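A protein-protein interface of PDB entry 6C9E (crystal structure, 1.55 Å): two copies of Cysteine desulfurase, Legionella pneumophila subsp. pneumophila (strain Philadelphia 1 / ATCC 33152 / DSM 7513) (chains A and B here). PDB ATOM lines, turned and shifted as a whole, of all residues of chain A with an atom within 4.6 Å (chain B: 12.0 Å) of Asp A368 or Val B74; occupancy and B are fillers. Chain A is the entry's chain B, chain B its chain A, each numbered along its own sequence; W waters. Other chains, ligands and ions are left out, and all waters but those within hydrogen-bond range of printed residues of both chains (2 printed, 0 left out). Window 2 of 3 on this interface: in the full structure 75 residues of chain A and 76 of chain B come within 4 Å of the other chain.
Ile A35 touches Ala B76.
Ile A35 touches Leu B77 (CD1 to CD1, 3.6 Å).
ND1 of His A361 touches CG1 of Val B74 (3.9 Å).
O of Gly A364 touches CG2 of Val B74, 3.7 Å away.
Val B74 touches Asp A368.
Asp A368 touches His B75 (OD1 to CA, 3.2 Å).
O of Ile A374 touches CG2 of Val B74, 3.7 Å away.
His B75 touches Ile A374.
Of the 12 printed residues of chain A, 5 touch a printed residue of chain B.
Among the printed residues, 9 pairs touch across the chains.
Among the printed residues, no Asp or Glu carboxylate lies within 4 Å of a Lys or Arg side-chain nitrogen of the other chain.
OD1 of Asp A368 is in hydrogen-bond range of N of Ala B76 (2.8 Å).
Water W2 lies within hydrogen-bond range of OD2 of Asp A368 (2.8 Å), O of Val B74 (3.3 Å) and N of Ala B76 (3.3 Å).
Water W1 lies within hydrogen-bond range of O of Ile A374 (2.8 Å) and N of Val B74 (2.9 Å).
Of the printed residues of chain B, Ile A35 touches Ala B76 and Leu B77.
Of chain B, only Val B74 (3.9 Å) comes within 4 Å of His A361.
Printed residues of chain B within 4 Å of Gly A364: Val B74.
Asp A368 touches three residues of chain B.
No residue of chain B comes within 4 Å of Ser A369.
No residue of chain B comes within 4 Å of Gly A371.
No residue of chain B comes within 4 Å of Ile A372.
Of the printed residues of chain A, Val B74 touches His A361, Gly A364, Asp A368 and Ile A374.
Printed residues of chain A within 4 Å of Leu B77: Ile A35.
The nearest printed residue of chain B that does not touch Asp A368 is Leu B77 (5.3 Å).
The nearest printed residue of chain A that does not touch Ala B76 is Ile A372 (6.6 Å).
N of Ser B78 is in hydrogen-bond range of ND1 of His B75, at 3.3 Å.
The backbone carbonyl oxygen (O) of His A361 sits at hydrogen-bond distance from the side-chain hydroxyl (OG1) of Thr A365 (2.9 Å).
No position is printed for both chains.
Of the 9 pairs that touch across the chains among the printed residues, none has its exchanged pair printed and touching as well.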
ATOM      1  N   ILE A  35      25.244  30.126  13.782  1.00  0.00           N
ATOM      2  CA  ILE A  35      24.138  30.637  12.989  1.00  0.00           C
ATOM      3  C   ILE A  35      24.061  32.106  13.355  1.00  0.00           C
ATOM      4  O   ILE A  35      23.569  32.449  14.434  1.00  0.00           O
ATOM      5  CB  ILE A  35      22.827  29.897  13.296  1.00  0.00           C
ATOM      6  CG1 ILE A  35      23.002  28.383  13.174  1.00  0.00           C
ATOM      7  CG2 ILE A  35      21.675  30.415  12.422  1.00  0.00           C
ATOM      8  CD1 ILE A  35      23.488  27.889  11.822  1.00  0.00           C
ATOM      9  N   HIS A 361       4.647  28.849  14.173  1.00  0.00           N
ATOM     10  CA  HIS A 361       5.627  29.350  13.207  1.00  0.00           C
ATOM     11  C   HIS A 361       6.501  30.431  13.823  1.00  0.00           C
ATOM     12  O   HIS A 361       7.706  30.491  13.556  1.00  0.00           O
ATOM     13  CB  HIS A 361       4.905  29.875  11.965  1.00  0.00           C
ATOM     14  CG  HIS A 361       5.808  30.521  10.953  1.00  0.00           C
ATOM     15  ND1 HIS A 361       6.555  29.798  10.044  1.00  0.00           N
ATOM     16  CD2 HIS A 361       6.064  31.826  10.694  1.00  0.00           C
ATOM     17  CE1 HIS A 361       7.243  30.630   9.278  1.00  0.00           C
ATOM     18  NE2 HIS A 361       6.965  31.866   9.654  1.00  0.00           N
ATOM     19  N   GLY A 364       9.127  28.801  16.135  1.00  0.00           N
ATOM     20  CA  GLY A 364      10.243  28.200  15.414  1.00  0.00           C
ATOM     21  C   GLY A 364      11.167  29.223  14.787  1.00  0.00           C
ATOM     22  O   GLY A 364      12.393  29.063  14.809  1.00  0.00           O
ATOM     23  N   THR A 365      10.600  30.293  14.215  1.00  0.00           N
ATOM     24  CA  THR A 365      11.399  31.341  13.579  1.00  0.00           C
ATOM     25  C   THR A 365      12.251  32.086  14.598  1.00  0.00           C
ATOM     26  O   THR A 365      13.430  32.367  14.366  1.00  0.00           O
ATOM     27  CB  THR A 365      10.467  32.321  12.850  1.00  0.00           C
ATOM     28  OG1 THR A 365       9.723  31.618  11.848  1.00  0.00           O
ATOM     29  CG2 THR A 365      11.254  33.445  12.196  1.00  0.00           C
ATOM     30  N   ILE A 366      11.645  32.460  15.736  1.00  0.00           N
ATOM     31  CA  ILE A 366      12.415  33.210  16.731  1.00  0.00           C
ATOM     32  C   ILE A 366      13.495  32.334  17.360  1.00  0.00           C
ATOM     33  O   ILE A 366      14.635  32.783  17.559  1.00  0.00           O
ATOM     34  CB  ILE A 366      11.483  33.835  17.788  1.00  0.00           C
ATOM     35  CG1 ILE A 366      10.560  34.862  17.126  1.00  0.00           C
ATOM     36  CG2 ILE A 366      12.315  34.502  18.882  1.00  0.00           C
ATOM     37  CD1 ILE A 366       9.386  35.245  18.011  1.00  0.00           C
ATOM     38  N   LEU A 367      13.197  31.052  17.608  1.00  0.00           N
ATOM     39  CA  LEU A 367      14.242  30.173  18.129  1.00  0.00           C
ATOM     40  C   LEU A 367      15.407  30.066  17.149  1.00  0.00           C
ATOM     41  O   LEU A 367      16.574  30.102  17.559  1.00  0.00           O
ATOM     42  CB  LEU A 367      13.667  28.795  18.457  1.00  0.00           C
ATOM     43  CG  LEU A 367      13.392  28.548  19.948  1.00  0.00           C
ATOM     44  CD1 LEU A 367      12.632  29.655  20.655  1.00  0.00           C
ATOM     45  CD2 LEU A 367      12.669  27.195  20.129  1.00  0.00           C
ATOM     46  N   ASP A 368      15.117  29.967  15.848  1.00  0.00           N
ATOM     47  CA  ASP A 368      16.204  29.903  14.881  1.00  0.00           C
ATOM     48  C   ASP A 368      17.034  31.175  14.878  1.00  0.00           C
ATOM     49  O   ASP A 368      18.230  31.129  14.573  1.00  0.00           O
ATOM     50  CB  ASP A 368      15.665  29.639  13.482  1.00  0.00           C
ATOM     51  CG  ASP A 368      16.754  29.773  12.431  1.00  0.00           C
ATOM     52  OD1 ASP A 368      17.643  28.889  12.387  1.00  0.00           O
ATOM     53  OD2 ASP A 368      16.743  30.784  11.691  1.00  0.00           O
ATOM     54  N   SER A 369      16.426  32.325  15.196  1.00  0.00           N
ATOM     55  CA  SER A 369      17.205  33.561  15.246  1.00  0.00           C
ATOM     56  C   SER A 369      18.263  33.519  16.338  1.00  0.00           C
ATOM     57  O   SER A 369      19.204  34.322  16.302  1.00  0.00           O
ATOM     58  CB  SER A 369      16.302  34.794  15.455  1.00  0.00           C
ATOM     59  OG  SER A 369      15.860  34.932  16.801  1.00  0.00           O
ATOM     60  N   GLU A 370      18.116  32.619  17.312  1.00  0.00           N
ATOM     61  CA  GLU A 370      19.123  32.375  18.339  1.00  0.00           C
ATOM     62  C   GLU A 370      19.862  31.060  18.102  1.00  0.00           C
ATOM     63  O   GLU A 370      20.435  30.491  19.041  1.00  0.00           O
ATOM     64  CB  GLU A 370      18.487  32.375  19.726  1.00  0.00           C
ATOM     65  CG  GLU A 370      17.821  33.701  20.102  1.00  0.00           C
ATOM     66  CD  GLU A 370      17.499  33.766  21.594  1.00  0.00           C
ATOM     67  OE1 GLU A 370      18.177  33.087  22.403  1.00  0.00           O
ATOM     68  OE2 GLU A 370      16.592  34.524  21.956  1.00  0.00           O
ATOM     69  N   GLY A 371      19.859  30.573  16.864  1.00  0.00           N
ATOM     70  CA  GLY A 371      20.617  29.390  16.479  1.00  0.00           C
ATOM     71  C   GLY A 371      19.939  28.062  16.737  1.00  0.00           C
ATOM     72  O   GLY A 371      20.527  27.008  16.408  1.00  0.00           O
ATOM     73  N   ILE A 372      18.725  28.059  17.282  1.00  0.00           N
ATOM     74  CA  ILE A 372      18.092  26.826  17.744  1.00  0.00           C
ATOM     75  C   ILE A 372      17.189  26.297  16.638  1.00  0.00           C
ATOM     76  O   ILE A 372      16.261  26.984  16.197  1.00  0.00           O
ATOM     77  CB  ILE A 372      17.289  27.066  19.029  1.00  0.00           C
ATOM     78  CG1 ILE A 372      18.196  27.588  20.135  1.00  0.00           C
ATOM     79  CG2 ILE A 372      16.575  25.770  19.431  1.00  0.00           C
ATOM     80  CD1 ILE A 372      17.432  28.400  21.166  1.00  0.00           C
ATOM     81  N   ILE A 374      14.383  23.874  15.442  1.00  0.00           N
ATOM     82  CA  ILE A 374      13.249  23.000  15.760  1.00  0.00           C
ATOM     83  C   ILE A 374      12.349  22.932  14.528  1.00  0.00           C
ATOM     84  O   ILE A 374      12.634  23.533  13.499  1.00  0.00           O
ATOM     85  CB  ILE A 374      12.464  23.471  17.005  1.00  0.00           C
ATOM     86  CG1 ILE A 374      11.811  24.836  16.763  1.00  0.00           C
ATOM     87  CG2 ILE A 374      13.378  23.497  18.221  1.00  0.00           C
ATOM     88  CD1 ILE A 374      10.569  25.024  17.650  1.00  0.00           C
ATOM     89  N   LYS B  65      28.434  20.410   6.754  1.00  0.00           N
ATOM     90  CA  LYS B  65      28.063  21.818   6.930  1.00  0.00           C
ATOM     91  C   LYS B  65      26.571  22.082   6.906  1.00  0.00           C
ATOM     92  O   LYS B  65      26.106  22.957   7.641  1.00  0.00           O
ATOM     93  CB  LYS B  65      28.725  22.662   5.810  1.00  0.00           C
ATOM     94  CG  LYS B  65      30.223  22.650   5.853  1.00  0.00           C
ATOM     95  CD  LYS B  65      30.808  23.741   4.972  1.00  0.00           C
ATOM     96  CE  LYS B  65      30.791  23.360   3.525  1.00  0.00           C
ATOM     97  NZ  LYS B  65      31.551  24.378   2.720  1.00  0.00           N
ATOM     98  N   ASP B  66      25.812  21.397   6.034  1.00  0.00           N
ATOM     99  CA  ASP B  66      24.487  21.894   5.660  1.00  0.00           C
ATOM    100  C   ASP B  66      23.350  20.925   5.936  1.00  0.00           C
ATOM    101  O   ASP B  66      22.185  21.290   5.719  1.00  0.00           O
ATOM    102  CB  ASP B  66      24.452  22.249   4.162  1.00  0.00           C
ATOM    103  CG  ASP B  66      25.466  23.330   3.809  1.00  0.00           C
ATOM    104  OD1 ASP B  66      25.538  24.352   4.544  1.00  0.00           O
ATOM    105  OD2 ASP B  66      26.217  23.127   2.825  1.00  0.00           O
ATOM    106  N   ASN B  67      23.647  19.704   6.372  1.00  0.00           N
ATOM    107  CA  ASN B  67      22.632  18.669   6.414  1.00  0.00           C
ATOM    108  C   ASN B  67      21.447  19.050   7.296  1.00  0.00           C
ATOM    109  O   ASN B  67      21.614  19.481   8.442  1.00  0.00           O
ATOM    110  CB  ASN B  67      23.267  17.383   6.919  1.00  0.00           C
ATOM    111  CG  ASN B  67      22.268  16.253   7.055  1.00  0.00           C
ATOM    112  OD1 ASN B  67      21.768  15.727   6.057  1.00  0.00           O
ATOM    113  ND2 ASN B  67      21.943  15.899   8.296  1.00  0.00           N
ATOM    114  N   SER B  68      20.252  18.814   6.755  1.00  0.00           N
ATOM    115  CA  SER B  68      18.945  18.997   7.380  1.00  0.00           C
ATOM    116  C   SER B  68      17.923  18.510   6.367  1.00  0.00           C
ATOM    117  O   SER B  68      18.249  18.278   5.197  1.00  0.00           O
ATOM    118  CB  SER B  68      18.666  20.457   7.795  1.00  0.00           C
ATOM    119  OG  SER B  68      19.194  20.745   9.096  1.00  0.00           O
ATOM    120  N   ASN B  69      16.690  18.332   6.823  1.00  0.00           N
ATOM    121  CA  ASN B  69      15.688  17.881   5.884  1.00  0.00           C
ATOM    122  C   ASN B  69      15.182  19.092   5.112  1.00  0.00           C
ATOM    123  O   ASN B  69      15.436  20.247   5.486  1.00  0.00           O
ATOM    124  CB  ASN B  69      14.566  17.112   6.601  1.00  0.00           C
ATOM    125  CG  ASN B  69      13.958  16.018   5.722  1.00  0.00           C
ATOM    126  OD1 ASN B  69      13.845  16.168   4.512  1.00  0.00           O
ATOM    127  ND2 ASN B  69      13.565  14.900   6.342  1.00  0.00           N
ATOM    128  N   VAL B  70      14.523  18.825   4.004  1.00  0.00           N
ATOM    129  CA  VAL B  70      14.189  19.871   3.043  1.00  0.00           C
ATOM    130  C   VAL B  70      12.687  20.119   3.034  1.00  0.00           C
ATOM    131  O   VAL B  70      11.872  19.208   3.250  1.00  0.00           O
ATOM    132  CB  VAL B  70      14.717  19.535   1.632  1.00  0.00           C
ATOM    133  CG1 VAL B  70      16.256  19.589   1.621  1.00  0.00           C
ATOM    134  CG2 VAL B  70      14.163  18.176   1.090  1.00  0.00           C
ATOM    135  N   HIS B  71      12.328  21.391   2.791  1.00  0.00           N
ATOM    136  CA  HIS B  71      10.969  21.920   2.681  1.00  0.00           C
ATOM    137  C   HIS B  71      10.291  22.079   4.036  1.00  0.00           C
ATOM    138  O   HIS B  71      10.578  21.344   4.983  1.00  0.00           O
ATOM    139  CB  HIS B  71      10.085  21.060   1.756  1.00  0.00           C
ATOM    140  CG  HIS B  71      10.686  20.823   0.411  1.00  0.00           C
ATOM    141  ND1 HIS B  71      11.035  19.562  -0.031  1.00  0.00           N
ATOM    142  CD2 HIS B  71      11.043  21.683  -0.574  1.00  0.00           C
ATOM    143  CE1 HIS B  71      11.554  19.656  -1.244  1.00  0.00           C
ATOM    144  NE2 HIS B  71      11.586  20.934  -1.591  1.00  0.00           N
ATOM    145  N   ARG B  72       9.410  23.071   4.127  1.00  0.00           N
ATOM    146  CA  ARG B  72       8.585  23.278   5.314  1.00  0.00           C
ATOM    147  C   ARG B  72       9.435  23.430   6.571  1.00  0.00           C
ATOM    148  O   ARG B  72       8.998  23.090   7.669  1.00  0.00           O
ATOM    149  CB  ARG B  72       7.558  22.150   5.470  1.00  0.00           C
ATOM    150  CG  ARG B  72       6.407  22.269   4.463  1.00  0.00           C
ATOM    151  CD  ARG B  72       5.603  20.974   4.293  1.00  0.00           C
ATOM    152  NE  ARG B  72       6.358  19.929   3.592  1.00  0.00           N
ATOM    153  CZ  ARG B  72       6.610  19.922   2.280  1.00  0.00           C
ATOM    154  NH1 ARG B  72       6.184  20.917   1.501  1.00  0.00           N
ATOM    155  NH2 ARG B  72       7.307  18.925   1.740  1.00  0.00           N
ATOM    156  N   GLY B  73      10.638  23.989   6.421  1.00  0.00           N
ATOM    157  CA  GLY B  73      11.510  24.209   7.561  1.00  0.00           C
ATOM    158  C   GLY B  73      11.626  25.676   7.916  1.00  0.00           C
ATOM    159  O   GLY B  73      11.355  26.563   7.094  1.00  0.00           O
ATOM    160  N   VAL B  74      11.978  25.946   9.163  1.00  0.00           N
ATOM    161  CA  VAL B  74      12.141  27.319   9.628  1.00  0.00           C
ATOM    162  C   VAL B  74      13.575  27.651   9.962  1.00  0.00           C
ATOM    163  O   VAL B  74      13.887  28.839  10.153  1.00  0.00           O
ATOM    164  CB  VAL B  74      11.241  27.632  10.846  1.00  0.00           C
ATOM    165  CG1 VAL B  74       9.767  27.591  10.448  1.00  0.00           C
ATOM    166  CG2 VAL B  74      11.536  26.697  12.040  1.00  0.00           C
ATOM    167  N   HIS B  75      14.459  26.668  10.043  1.00  0.00           N
ATOM    168  CA  HIS B  75      15.761  26.947  10.617  1.00  0.00           C
ATOM    169  C   HIS B  75      16.829  26.975   9.532  1.00  0.00           C
ATOM    170  O   HIS B  75      16.637  26.499   8.413  1.00  0.00           O
ATOM    171  CB  HIS B  75      16.103  25.950  11.748  1.00  0.00           C
ATOM    172  CG  HIS B  75      16.121  24.497  11.352  1.00  0.00           C
ATOM    173  ND1 HIS B  75      17.157  23.920  10.646  1.00  0.00           N
ATOM    174  CD2 HIS B  75      15.253  23.491  11.638  1.00  0.00           C
ATOM    175  CE1 HIS B  75      16.924  22.628  10.500  1.00  0.00           C
ATOM    176  NE2 HIS B  75      15.771  22.342  11.082  1.00  0.00           N
ATOM    177  N   ALA B  76      17.958  27.588   9.891  1.00  0.00           N
ATOM    178  CA  ALA B  76      18.959  27.997   8.906  1.00  0.00           C
ATOM    179  C   ALA B  76      19.452  26.839   8.049  1.00  0.00           C
ATOM    180  O   ALA B  76      19.545  26.962   6.825  1.00  0.00           O
ATOM    181  CB  ALA B  76      20.133  28.666   9.623  1.00  0.00           C
ATOM    182  N   LEU B  77      19.807  25.714   8.667  1.00  0.00           N
ATOM    183  CA  LEU B  77      20.322  24.615   7.854  1.00  0.00           C
ATOM    184  C   LEU B  77      19.239  24.041   6.951  1.00  0.00           C
ATOM    185  O   LEU B  77      19.522  23.681   5.805  1.00  0.00           O
ATOM    186  CB  LEU B  77      20.941  23.515   8.725  1.00  0.00           C
ATOM    187  CG  LEU B  77      22.438  23.697   9.021  1.00  0.00           C
ATOM    188  CD1 LEU B  77      22.727  24.967   9.840  1.00  0.00           C
ATOM    189  CD2 LEU B  77      22.982  22.471   9.738  1.00  0.00           C
ATOM    190  N   SER B  78      17.994  23.939   7.428  1.00  0.00           N
ATOM    191  CA  SER B  78      16.937  23.450   6.547  1.00  0.00           C
ATOM    192  C   SER B  78      16.737  24.382   5.364  1.00  0.00           C
ATOM    193  O   SER B  78      16.565  23.927   4.228  1.00  0.00           O
ATOM    194  CB  SER B  78      15.624  23.306   7.300  1.00  0.00           C
ATOM    195  OG  SER B  78      14.640  22.871   6.372  1.00  0.00           O
ATOM    196  N   VAL B  79      16.762  25.692   5.608  1.00  0.00           N
ATOM    197  CA  VAL B  79      16.631  26.655   4.524  1.00  0.00           C
ATOM    198  C   VAL B  79      17.777  26.489   3.530  1.00  0.00           C
ATOM    199  O   VAL B  79      17.549  26.446   2.309  1.00  0.00           O
ATOM    200  CB  VAL B  79      16.546  28.079   5.094  1.00  0.00           C
ATOM    201  CG1 VAL B  79      16.672  29.138   3.976  1.00  0.00           C
ATOM    202  CG2 VAL B  79      15.244  28.232   5.802  1.00  0.00           C
ATOM    203  N   ARG B  80      19.015  26.332   4.030  1.00  0.00           N
ATOM    204  CA  ARG B  80      20.172  26.181   3.141  1.00  0.00           C
ATOM    205  C   ARG B  80      20.056  24.899   2.345  1.00  0.00           C
ATOM    206  O   ARG B  80      20.249  24.898   1.122  1.00  0.00           O
ATOM    207  CB  ARG B  80      21.495  26.144   3.924  1.00  0.00           C
ATOM    208  CG  ARG B  80      21.859  27.416   4.646  1.00  0.00           C
ATOM    209  CD  ARG B  80      23.362  27.551   4.782  1.00  0.00           C
ATOM    210  NE  ARG B  80      24.088  26.535   5.557  1.00  0.00           N
ATOM    211  CZ  ARG B  80      24.567  26.729   6.789  1.00  0.00           C
ATOM    212  NH1 ARG B  80      24.312  27.860   7.444  1.00  0.00           N
ATOM    213  NH2 ARG B  80      25.317  25.790   7.367  1.00  0.00           N
ATOM    214  N   ALA B  81      19.747  23.790   3.032  1.00  0.00           N
ATOM    215  CA  ALA B  81      19.678  22.499   2.352  1.00  0.00           C
ATOM    216  C   ALA B  81      18.586  22.499   1.296  1.00  0.00           C
ATOM    217  O   ALA B  81      18.743  21.896   0.223  1.00  0.00           O
ATOM    218  CB  ALA B  81      19.435  21.391   3.373  1.00  0.00           C
ATOM    219  N   THR B  82      17.444  23.125   1.606  1.00  0.00           N
ATOM    220  CA  THR B  82      16.350  23.168   0.639  1.00  0.00           C
ATOM    221  C   THR B  82      16.746  23.959  -0.591  1.00  0.00           C
ATOM    222  O   THR B  82      16.465  23.541  -1.716  1.00  0.00           O
ATOM    223  CB  THR B  82      15.115  23.795   1.274  1.00  0.00           C
ATOM    224  OG1 THR B  82      14.757  23.040   2.432  1.00  0.00           O
ATOM    225  CG2 THR B  82      13.957  23.779   0.297  1.00  0.00           C
ATOM    226  N   GLU B  83      17.418  25.101  -0.403  1.00  0.00           N
ATOM    227  CA  GLU B  83      17.881  25.859  -1.563  1.00  0.00           C
ATOM    228  C   GLU B  83      18.853  25.035  -2.398  1.00  0.00           C
ATOM    229  O   GLU B  83      18.796  25.054  -3.633  1.00  0.00           O
ATOM    230  CB  GLU B  83      18.517  27.193  -1.136  1.00  0.00           C
ATOM    231  CG  GLU B  83      19.206  27.999  -2.279  1.00  0.00           C
ATOM    232  CD  GLU B  83      18.271  28.661  -3.307  1.00  0.00           C
ATOM    233  OE1 GLU B  83      17.039  28.609  -3.118  1.00  0.00           O
ATOM    234  OE2 GLU B  83      18.785  29.220  -4.329  1.00  0.00           O
ATOM    235  N   GLU B 270       5.322  14.622   2.113  1.00  0.00           N
ATOM    236  CA  GLU B 270       5.993  15.539   1.188  1.00  0.00           C
ATOM    237  C   GLU B 270       5.306  15.640  -0.170  1.00  0.00           C
ATOM    238  O   GLU B 270       5.382  16.691  -0.816  1.00  0.00           O
ATOM    239  CB  GLU B 270       7.472  15.165   0.977  1.00  0.00           C
ATOM    240  CG  GLU B 270       8.261  14.769   2.250  1.00  0.00           C
ATOM    241  CD  GLU B 270       8.206  15.823   3.334  1.00  0.00           C
ATOM    242  OE1 GLU B 270       8.203  15.441   4.522  1.00  0.00           O
ATOM    243  OE2 GLU B 270       8.174  17.028   3.006  1.00  0.00           O
HETATM  244  O   HOH W   1      12.148  23.572  10.740  1.00  0.00           O
HETATM  245  O   HOH W   2      16.526  30.413   8.944  1.00  0.00           O
